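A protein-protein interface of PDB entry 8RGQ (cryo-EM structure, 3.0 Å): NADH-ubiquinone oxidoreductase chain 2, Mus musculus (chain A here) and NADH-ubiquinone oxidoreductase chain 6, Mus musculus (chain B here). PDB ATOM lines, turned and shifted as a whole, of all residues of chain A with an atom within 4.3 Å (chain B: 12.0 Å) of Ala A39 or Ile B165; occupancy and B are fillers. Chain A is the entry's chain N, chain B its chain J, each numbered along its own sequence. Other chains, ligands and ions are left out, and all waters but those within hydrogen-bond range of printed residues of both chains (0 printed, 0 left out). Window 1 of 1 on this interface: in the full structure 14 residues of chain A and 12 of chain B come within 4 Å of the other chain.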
ATOM      1  N   ILE A   9      15.058  -6.256   0.747  1.00  0.00           N
ATOM      2  CA  ILE A   9      15.771  -4.985   0.690  1.00  0.00           C
ATOM      3  C   ILE A   9      16.540  -4.736   1.984  1.00  0.00           C
ATOM      4  O   ILE A   9      17.715  -4.350   1.951  1.00  0.00           O
ATOM      5  CB  ILE A   9      14.790  -3.841   0.373  1.00  0.00           C
ATOM      6  CG1 ILE A   9      14.412  -3.867  -1.109  1.00  0.00           C
ATOM      7  CG2 ILE A   9      15.384  -2.495   0.723  1.00  0.00           C
ATOM      8  CD1 ILE A   9      13.323  -2.888  -1.478  1.00  0.00           C
ATOM      9  N   THR A  12      19.564  -7.074   2.106  1.00  0.00           N
ATOM     10  CA  THR A  12      20.679  -6.654   1.260  1.00  0.00           C
ATOM     11  C   THR A  12      21.358  -5.401   1.812  1.00  0.00           C
ATOM     12  O   THR A  12      22.586  -5.262   1.714  1.00  0.00           O
ATOM     13  CB  THR A  12      20.196  -6.439  -0.172  1.00  0.00           C
ATOM     14  OG1 THR A  12      19.317  -7.508  -0.544  1.00  0.00           O
ATOM     15  CG2 THR A  12      21.373  -6.411  -1.134  1.00  0.00           C
ATOM     16  N   ILE A  13      20.575  -4.489   2.407  1.00  0.00           N
ATOM     17  CA  ILE A  13      21.138  -3.324   3.092  1.00  0.00           C
ATOM     18  C   ILE A  13      22.053  -3.765   4.225  1.00  0.00           C
ATOM     19  O   ILE A  13      23.152  -3.226   4.405  1.00  0.00           O
ATOM     20  CB  ILE A  13      20.010  -2.402   3.602  1.00  0.00           C
ATOM     21  CG1 ILE A  13      19.383  -1.612   2.457  1.00  0.00           C
ATOM     22  CG2 ILE A  13      20.512  -1.436   4.664  1.00  0.00           C
ATOM     23  CD1 ILE A  13      18.135  -0.854   2.849  1.00  0.00           C
ATOM     24  N   PHE A  35      26.053  -3.357  -3.210  1.00  0.00           N
ATOM     25  CA  PHE A  35      24.880  -3.914  -2.524  1.00  0.00           C
ATOM     26  C   PHE A  35      24.242  -2.878  -1.613  1.00  0.00           C
ATOM     27  O   PHE A  35      23.017  -2.705  -1.630  1.00  0.00           O
ATOM     28  CB  PHE A  35      25.140  -5.190  -1.705  1.00  0.00           C
ATOM     29  CG  PHE A  35      25.471  -6.421  -2.507  1.00  0.00           C
ATOM     30  CD1 PHE A  35      24.452  -7.135  -3.114  1.00  0.00           C
ATOM     31  CD2 PHE A  35      26.723  -6.994  -2.465  1.00  0.00           C
ATOM     32  CE1 PHE A  35      24.713  -8.298  -3.818  1.00  0.00           C
ATOM     33  CE2 PHE A  35      26.996  -8.163  -3.162  1.00  0.00           C
ATOM     34  CZ  PHE A  35      25.982  -8.819  -3.830  1.00  0.00           C
ATOM     35  N   SER A  36      25.061  -2.153  -0.841  1.00  0.00           N
ATOM     36  CA  SER A  36      24.519  -1.115   0.035  1.00  0.00           C
ATOM     37  C   SER A  36      23.797  -0.032  -0.766  1.00  0.00           C
ATOM     38  O   SER A  36      22.646   0.313  -0.465  1.00  0.00           O
ATOM     39  CB  SER A  36      25.636  -0.504   0.878  1.00  0.00           C
ATOM     40  OG  SER A  36      26.684  -0.024   0.056  1.00  0.00           O
ATOM     41  N   LEU A  37      24.439   0.464  -1.828  1.00  0.00           N
ATOM     42  CA  LEU A  37      23.859   1.545  -2.627  1.00  0.00           C
ATOM     43  C   LEU A  37      22.570   1.112  -3.326  1.00  0.00           C
ATOM     44  O   LEU A  37      21.524   1.775  -3.200  1.00  0.00           O
ATOM     45  CB  LEU A  37      24.884   2.022  -3.656  1.00  0.00           C
ATOM     46  CG  LEU A  37      24.357   2.828  -4.843  1.00  0.00           C
ATOM     47  CD1 LEU A  37      23.873   4.191  -4.391  1.00  0.00           C
ATOM     48  CD2 LEU A  37      25.410   2.948  -5.929  1.00  0.00           C
ATOM     49  N   LEU A  38      22.629  -0.002  -4.069  1.00  0.00           N
ATOM     50  CA  LEU A  38      21.480  -0.475  -4.825  1.00  0.00           C
ATOM     51  C   LEU A  38      20.329  -0.856  -3.913  1.00  0.00           C
ATOM     52  O   LEU A  38      19.177  -0.555  -4.231  1.00  0.00           O
ATOM     53  CB  LEU A  38      21.871  -1.669  -5.696  1.00  0.00           C
ATOM     54  CG  LEU A  38      22.305  -1.399  -7.139  1.00  0.00           C
ATOM     55  CD1 LEU A  38      23.646  -0.692  -7.206  1.00  0.00           C
ATOM     56  CD2 LEU A  38      22.348  -2.702  -7.921  1.00  0.00           C
ATOM     57  N   ALA A  39      20.616  -1.487  -2.771  1.00  0.00           N
ATOM     58  CA  ALA A  39      19.545  -1.879  -1.871  1.00  0.00           C
ATOM     59  C   ALA A  39      18.923  -0.681  -1.170  1.00  0.00           C
ATOM     60  O   ALA A  39      17.725  -0.702  -0.869  1.00  0.00           O
ATOM     61  CB  ALA A  39      20.074  -2.877  -0.853  1.00  0.00           C
ATOM     62  N   ILE A  40      19.700   0.371  -0.902  1.00  0.00           N
ATOM     63  CA  ILE A  40      19.125   1.502  -0.189  1.00  0.00           C
ATOM     64  C   ILE A  40      18.380   2.475  -1.102  1.00  0.00           C
ATOM     65  O   ILE A  40      17.516   3.215  -0.613  1.00  0.00           O
ATOM     66  CB  ILE A  40      20.210   2.234   0.628  1.00  0.00           C
ATOM     67  CG1 ILE A  40      19.580   2.980   1.805  1.00  0.00           C
ATOM     68  CG2 ILE A  40      21.006   3.183  -0.233  1.00  0.00           C
ATOM     69  CD1 ILE A  40      20.570   3.664   2.692  1.00  0.00           C
ATOM     70  N   ILE A  41      18.654   2.469  -2.416  1.00  0.00           N
ATOM     71  CA  ILE A  41      17.979   3.417  -3.323  1.00  0.00           C
ATOM     72  C   ILE A  41      16.450   3.300  -3.344  1.00  0.00           C
ATOM     73  O   ILE A  41      15.775   4.345  -3.280  1.00  0.00           O
ATOM     74  CB  ILE A  41      18.614   3.347  -4.723  1.00  0.00           C
ATOM     75  CG1 ILE A  41      19.900   4.175  -4.733  1.00  0.00           C
ATOM     76  CG2 ILE A  41      17.662   3.832  -5.804  1.00  0.00           C
ATOM     77  CD1 ILE A  41      20.592   4.230  -6.058  1.00  0.00           C
ATOM     78  N   PRO A  42      15.835   2.098  -3.418  1.00  0.00           N
ATOM     79  CA  PRO A  42      14.362   2.048  -3.313  1.00  0.00           C
ATOM     80  C   PRO A  42      13.828   2.562  -1.996  1.00  0.00           C
ATOM     81  O   PRO A  42      12.693   3.051  -1.935  1.00  0.00           O
ATOM     82  CB  PRO A  42      14.038   0.559  -3.486  1.00  0.00           C
ATOM     83  CG  PRO A  42      15.168   0.010  -4.154  1.00  0.00           C
ATOM     84  CD  PRO A  42      16.353   0.739  -3.650  1.00  0.00           C
ATOM     85  N   MET A  43      14.620   2.454  -0.935  1.00  0.00           N
ATOM     86  CA  MET A  43      14.213   2.983   0.355  1.00  0.00           C
ATOM     87  C   MET A  43      14.211   4.508   0.373  1.00  0.00           C
ATOM     88  O   MET A  43      13.391   5.111   1.075  1.00  0.00           O
ATOM     89  CB  MET A  43      15.129   2.409   1.430  1.00  0.00           C
ATOM     90  CG  MET A  43      14.873   0.956   1.833  1.00  0.00           C
ATOM     91  SD  MET A  43      13.174   0.339   1.977  1.00  0.00           S
ATOM     92  CE  MET A  43      12.377   1.536   3.058  1.00  0.00           C
ATOM     93  N   VAL B 154      27.109 -14.198  -4.992  1.00  0.00           N
ATOM     94  CA  VAL B 154      26.902 -12.754  -4.907  1.00  0.00           C
ATOM     95  C   VAL B 154      26.369 -12.213  -6.226  1.00  0.00           C
ATOM     96  O   VAL B 154      25.546 -11.294  -6.224  1.00  0.00           O
ATOM     97  CB  VAL B 154      28.161 -11.984  -4.447  1.00  0.00           C
ATOM     98  CG1 VAL B 154      28.573 -12.410  -3.045  1.00  0.00           C
ATOM     99  CG2 VAL B 154      29.312 -12.094  -5.439  1.00  0.00           C
ATOM    100  N   ALA B 155      26.774 -12.790  -7.365  1.00  0.00           N
ATOM    101  CA  ALA B 155      26.183 -12.359  -8.630  1.00  0.00           C
ATOM    102  C   ALA B 155      24.709 -12.749  -8.715  1.00  0.00           C
ATOM    103  O   ALA B 155      23.867 -11.938  -9.136  1.00  0.00           O
ATOM    104  CB  ALA B 155      26.973 -12.942  -9.800  1.00  0.00           C
ATOM    105  N   GLY B 156      24.374 -13.971  -8.285  1.00  0.00           N
ATOM    106  CA  GLY B 156      22.979 -14.388  -8.293  1.00  0.00           C
ATOM    107  C   GLY B 156      22.106 -13.565  -7.363  1.00  0.00           C
ATOM    108  O   GLY B 156      20.998 -13.157  -7.731  1.00  0.00           O
ATOM    109  N   TRP B 157      22.598 -13.296  -6.150  1.00  0.00           N
ATOM    110  CA  TRP B 157      21.851 -12.465  -5.217  1.00  0.00           C
ATOM    111  C   TRP B 157      21.753 -11.029  -5.699  1.00  0.00           C
ATOM    112  O   TRP B 157      20.742 -10.367  -5.444  1.00  0.00           O
ATOM    113  CB  TRP B 157      22.487 -12.498  -3.831  1.00  0.00           C
ATOM    114  CG  TRP B 157      21.675 -11.737  -2.847  1.00  0.00           C
ATOM    115  CD1 TRP B 157      21.921 -10.483  -2.373  1.00  0.00           C
ATOM    116  CD2 TRP B 157      20.453 -12.162  -2.243  1.00  0.00           C
ATOM    117  NE1 TRP B 157      20.935 -10.108  -1.496  1.00  0.00           N
ATOM    118  CE2 TRP B 157      20.020 -11.123  -1.399  1.00  0.00           C
ATOM    119  CE3 TRP B 157      19.686 -13.327  -2.326  1.00  0.00           C
ATOM    120  CZ2 TRP B 157      18.857 -11.213  -0.647  1.00  0.00           C
ATOM    121  CZ3 TRP B 157      18.534 -13.414  -1.577  1.00  0.00           C
ATOM    122  CH2 TRP B 157      18.132 -12.366  -0.746  1.00  0.00           C
ATOM    123  N   SER B 158      22.781 -10.534  -6.394  1.00  0.00           N
ATOM    124  CA  SER B 158      22.705  -9.208  -6.991  1.00  0.00           C
ATOM    125  C   SER B 158      21.580  -9.134  -8.004  1.00  0.00           C
ATOM    126  O   SER B 158      20.817  -8.166  -8.020  1.00  0.00           O
ATOM    127  CB  SER B 158      24.033  -8.858  -7.653  1.00  0.00           C
ATOM    128  OG  SER B 158      23.972  -7.585  -8.269  1.00  0.00           O
ATOM    129  N   LEU B 159      21.434 -10.169  -8.831  1.00  0.00           N
ATOM    130  CA  LEU B 159      20.370 -10.151  -9.832  1.00  0.00           C
ATOM    131  C   LEU B 159      18.984 -10.293  -9.203  1.00  0.00           C
ATOM    132  O   LEU B 159      18.036  -9.608  -9.614  1.00  0.00           O
ATOM    133  CB  LEU B 159      20.625 -11.240 -10.863  1.00  0.00           C
ATOM    134  CG  LEU B 159      21.722 -10.717 -11.784  1.00  0.00           C
ATOM    135  CD1 LEU B 159      22.639 -11.820 -12.254  1.00  0.00           C
ATOM    136  CD2 LEU B 159      21.088  -9.991 -12.944  1.00  0.00           C
ATOM    137  N   PHE B 160      18.848 -11.168  -8.203  1.00  0.00           N
ATOM    138  CA  PHE B 160      17.567 -11.340  -7.516  1.00  0.00           C
ATOM    139  C   PHE B 160      17.146 -10.060  -6.796  1.00  0.00           C
ATOM    140  O   PHE B 160      16.007  -9.577  -6.944  1.00  0.00           O
ATOM    141  CB  PHE B 160      17.687 -12.507  -6.535  1.00  0.00           C
ATOM    142  CG  PHE B 160      16.377 -13.065  -6.073  1.00  0.00           C
ATOM    143  CD1 PHE B 160      15.511 -13.670  -6.967  1.00  0.00           C
ATOM    144  CD2 PHE B 160      16.030 -13.021  -4.734  1.00  0.00           C
ATOM    145  CE1 PHE B 160      14.310 -14.197  -6.536  1.00  0.00           C
ATOM    146  CE2 PHE B 160      14.833 -13.548  -4.296  1.00  0.00           C
ATOM    147  CZ  PHE B 160      13.971 -14.140  -5.199  1.00  0.00           C
ATOM    148  N   ALA B 161      18.074  -9.479  -6.032  1.00  0.00           N
ATOM    149  CA  ALA B 161      17.808  -8.217  -5.359  1.00  0.00           C
ATOM    150  C   ALA B 161      17.553  -7.105  -6.363  1.00  0.00           C
ATOM    151  O   ALA B 161      16.739  -6.221  -6.106  1.00  0.00           O
ATOM    152  CB  ALA B 161      18.971  -7.858  -4.438  1.00  0.00           C
ATOM    153  N   GLY B 162      18.220  -7.145  -7.519  1.00  0.00           N
ATOM    154  CA  GLY B 162      17.977  -6.142  -8.541  1.00  0.00           C
ATOM    155  C   GLY B 162      16.580  -6.227  -9.118  1.00  0.00           C
ATOM    156  O   GLY B 162      15.967  -5.201  -9.419  1.00  0.00           O
ATOM    157  N   ILE B 163      16.057  -7.447  -9.275  1.00  0.00           N
ATOM    158  CA  ILE B 163      14.653  -7.617  -9.658  1.00  0.00           C
ATOM    159  C   ILE B 163      13.746  -6.947  -8.632  1.00  0.00           C
ATOM    160  O   ILE B 163      12.875  -6.131  -8.977  1.00  0.00           O
ATOM    161  CB  ILE B 163      14.307  -9.111  -9.801  1.00  0.00           C
ATOM    162  CG1 ILE B 163      15.005  -9.730 -11.011  1.00  0.00           C
ATOM    163  CG2 ILE B 163      12.800  -9.304  -9.900  1.00  0.00           C
ATOM    164  CD1 ILE B 163      14.743 -11.206 -11.175  1.00  0.00           C
ATOM    165  N   PHE B 164      13.968  -7.262  -7.350  1.00  0.00           N
ATOM    166  CA  PHE B 164      13.125  -6.707  -6.287  1.00  0.00           C
ATOM    167  C   PHE B 164      13.201  -5.182  -6.255  1.00  0.00           C
ATOM    168  O   PHE B 164      12.172  -4.496  -6.180  1.00  0.00           O
ATOM    169  CB  PHE B 164      13.546  -7.295  -4.940  1.00  0.00           C
ATOM    170  CG  PHE B 164      12.931  -8.630  -4.642  1.00  0.00           C
ATOM    171  CD1 PHE B 164      13.223  -9.733  -5.425  1.00  0.00           C
ATOM    172  CD2 PHE B 164      12.092  -8.792  -3.557  1.00  0.00           C
ATOM    173  CE1 PHE B 164      12.664 -10.957  -5.151  1.00  0.00           C
ATOM    174  CE2 PHE B 164      11.523 -10.016  -3.283  1.00  0.00           C
ATOM    175  CZ  PHE B 164      11.816 -11.101  -4.076  1.00  0.00           C
ATOM    176  N   ILE B 165      14.415  -4.650  -6.392  1.00  0.00           N
ATOM    177  CA  ILE B 165      14.675  -3.214  -6.422  1.00  0.00           C
ATOM    178  C   ILE B 165      13.972  -2.545  -7.596  1.00  0.00           C
ATOM    179  O   ILE B 165      13.369  -1.480  -7.442  1.00  0.00           O
ATOM    180  CB  ILE B 165      16.200  -2.989  -6.455  1.00  0.00           C
ATOM    181  CG1 ILE B 165      16.817  -3.283  -5.084  1.00  0.00           C
ATOM    182  CG2 ILE B 165      16.562  -1.624  -6.997  1.00  0.00           C
ATOM    183  CD1 ILE B 165      18.305  -3.491  -5.134  1.00  0.00           C
ATOM    184  N   ILE B 166      14.034  -3.154  -8.782  1.00  0.00           N
ATOM    185  CA  ILE B 166      13.519  -2.494  -9.977  1.00  0.00           C
ATOM    186  C   ILE B 166      11.996  -2.430  -9.956  1.00  0.00           C
ATOM    187  O   ILE B 166      11.408  -1.373 -10.227  1.00  0.00           O
ATOM    188  CB  ILE B 166      14.052  -3.189 -11.240  1.00  0.00           C
ATOM    189  CG1 ILE B 166      15.505  -2.769 -11.462  1.00  0.00           C
ATOM    190  CG2 ILE B 166      13.197  -2.853 -12.449  1.00  0.00           C
ATOM    191  CD1 ILE B 166      15.690  -1.275 -11.609  1.00  0.00           C
ATOM    192  N   ILE B 167      11.330  -3.546  -9.629  1.00  0.00           N
ATOM    193  CA  ILE B 167       9.871  -3.462  -9.493  1.00  0.00           C
ATOM    194  C   ILE B 167       9.457  -2.559  -8.329  1.00  0.00           C
ATOM    195  O   ILE B 167       8.460  -1.831  -8.437  1.00  0.00           O
ATOM    196  CB  ILE B 167       9.189  -4.858  -9.457  1.00  0.00           C
ATOM    197  CG1 ILE B 167       9.365  -5.621 -10.784  1.00  0.00           C
ATOM    198  CG2 ILE B 167       7.700  -4.780  -9.147  1.00  0.00           C
ATOM    199  CD1 ILE B 167      10.549  -6.485 -10.976  1.00  0.00           C
ATOM    200  N   GLU B 168      10.235  -2.512  -7.241  1.00  0.00           N
ATOM    201  CA  GLU B 168       9.871  -1.598  -6.159  1.00  0.00           C
ATOM    202  C   GLU B 168      10.022  -0.131  -6.569  1.00  0.00           C
ATOM    203  O   GLU B 168       9.178   0.703  -6.220  1.00  0.00           O
ATOM    204  CB  GLU B 168      10.695  -1.894  -4.907  1.00  0.00           C
ATOM    205  CG  GLU B 168      10.327  -1.002  -3.732  1.00  0.00           C
ATOM    206  CD  GLU B 168       8.904  -1.233  -3.237  1.00  0.00           C
ATOM    207  OE1 GLU B 168       8.366  -2.347  -3.420  1.00  0.00           O
ATOM    208  OE2 GLU B 168       8.304  -0.284  -2.693  1.00  0.00           O
ATOM    209  N   ILE B 169      11.076   0.201  -7.318  1.00  0.00           N
ATOM    210  CA  ILE B 169      11.286   1.583  -7.746  1.00  0.00           C
ATOM    211  C   ILE B 169      10.229   1.996  -8.762  1.00  0.00           C
ATOM    212  O   ILE B 169       9.616   3.065  -8.647  1.00  0.00           O
ATOM    213  CB  ILE B 169      12.708   1.762  -8.309  1.00  0.00           C
ATOM    214  CG1 ILE B 169      13.738   1.766  -7.183  1.00  0.00           C
ATOM    215  CG2 ILE B 169      12.822   3.057  -9.093  1.00  0.00           C
ATOM    216  CD1 ILE B 169      15.161   1.761  -7.679  1.00  0.00           C
ATOM    217  N   THR B 170       9.976   1.149  -9.756  1.00  0.00           N
ATOM    218  CA  THR B 170       9.032   1.471 -10.815  1.00  0.00           C
ATOM    219  C   THR B 170       7.592   1.139 -10.445  1.00  0.00           C
ATOM    220  O   THR B 170       6.712   1.228 -11.307  1.00  0.00           O
ATOM    221  CB  THR B 170       9.417   0.738 -12.099  1.00  0.00           C
ATOM    222  OG1 THR B 170       9.367  -0.674 -11.872  1.00  0.00           O
ATOM    223  CG2 THR B 170      10.822   1.125 -12.525  1.00  0.00           C
ATOM    224  N   ARG B 171       7.342   0.740  -9.194  1.00  0.00           N
ATOM    225  CA  ARG B 171       5.978   0.465  -8.752  1.00  0.00           C
ATOM    226  C   ARG B 171       5.113   1.720  -8.789  1.00  0.00           C
ATOM    227  O   ARG B 171       3.947   1.660  -9.198  1.00  0.00           O
ATOM    228  CB  ARG B 171       6.002  -0.130  -7.344  1.00  0.00           C
ATOM    229  CG  ARG B 171       4.641  -0.516  -6.801  1.00  0.00           C
ATOM    230  CD  ARG B 171       4.761  -1.107  -5.406  1.00  0.00           C
ATOM    231  NE  ARG B 171       5.292  -0.143  -4.451  1.00  0.00           N
ATOM    232  CZ  ARG B 171       4.567   0.777  -3.829  1.00  0.00           C
ATOM    233  NH1 ARG B 171       3.264   0.887  -4.036  1.00  0.00           N
ATOM    234  NH2 ARG B 171       5.161   1.607  -2.978  1.00  0.00           N
ATOM    235  N   ASP B 172       5.673   2.857  -8.371  1.00  0.00           N
ATOM    236  CA  ASP B 172       5.005   4.165  -8.358  1.00  0.00           C
ATOM    237  C   ASP B 172       3.687   4.161  -7.582  1.00  0.00           C
ATOM    238  O   ASP B 172       3.403   5.081  -6.815  1.00  0.00           O
ATOM    239  CB  ASP B 172       4.765   4.662  -9.788  1.00  0.00           C
ATOM    240  CG  ASP B 172       3.889   5.898  -9.837  1.00  0.00           C
ATOM    241  OD1 ASP B 172       4.369   6.984  -9.452  1.00  0.00           O
ATOM    242  OD2 ASP B 172       2.719   5.781 -10.259  1.00  0.00           O
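Of the 12 printed residues of chain A, 6 touch a printed residue of chain B.
Hydrophobic or aromatic side chains of chain A that line the printed part of chain B: Phe A35, Ile A41 and Pro A42.
The indole nitrogen (NE1) of Trp B157 is in hydrogen-bond range of the side-chain hydroxyl (OG1) of Thr A12 (3.2 Å).
Ala A39 touches one residue of chain B.
Of chain A, only Leu A38 (3.2 Å), Ala A39 (3.8 Å) and Pro A42 (3.6 Å) come within 4 Å of Ile B165.
No residue of chain B comes within 4 Å of Ile A9.
Of chain B, only Trp B157 (3.2 Å) and Ala B161 (3.9 Å) come within 4 Å of Thr A12.
No residue of chain B comes within 4 Å of Ile A13.
Leu A37 touches none of the printed residues of chain B.
Of chain B, only Ile B165 (3.2 Å) comes within 4 Å of Leu A38.
Of chain B, only Ile B165 (3.6 Å) and Ile B169 (3.8 Å) come within 4 Å of Pro A42.
Printed residues of chain A within 4 Å of Ala B161: Thr A12.
Printed residues of chain A within 4 Å of Val B154: Phe A35 (3.5 Å).
Gly B162 touches none of the printed residues of chain A.
The nearest printed residue of chain A that does not touch Ile B165 is Ile A9 (4.7 Å).
Thr A12 touches Ala B161 (OG1 to CB, 3.9 Å).
Phe A35 touches Val B154 (CZ to O, 3.5 Å).
Phe A35 touches Trp B157.
Ser B158 touches Phe A35.
O of Leu A38 touches CD1 of Ile B165 (3.2 Å).
Ile B165 touches Ala A39 (CD1 to CA, 3.8 Å).
Ile B169 touches Ile A41.
Pro A42 touches Ile B165 (CG to CG2, 3.6 Å).
CG1 of Ile B169 touches CG of Pro A42, at 3.8 Å.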
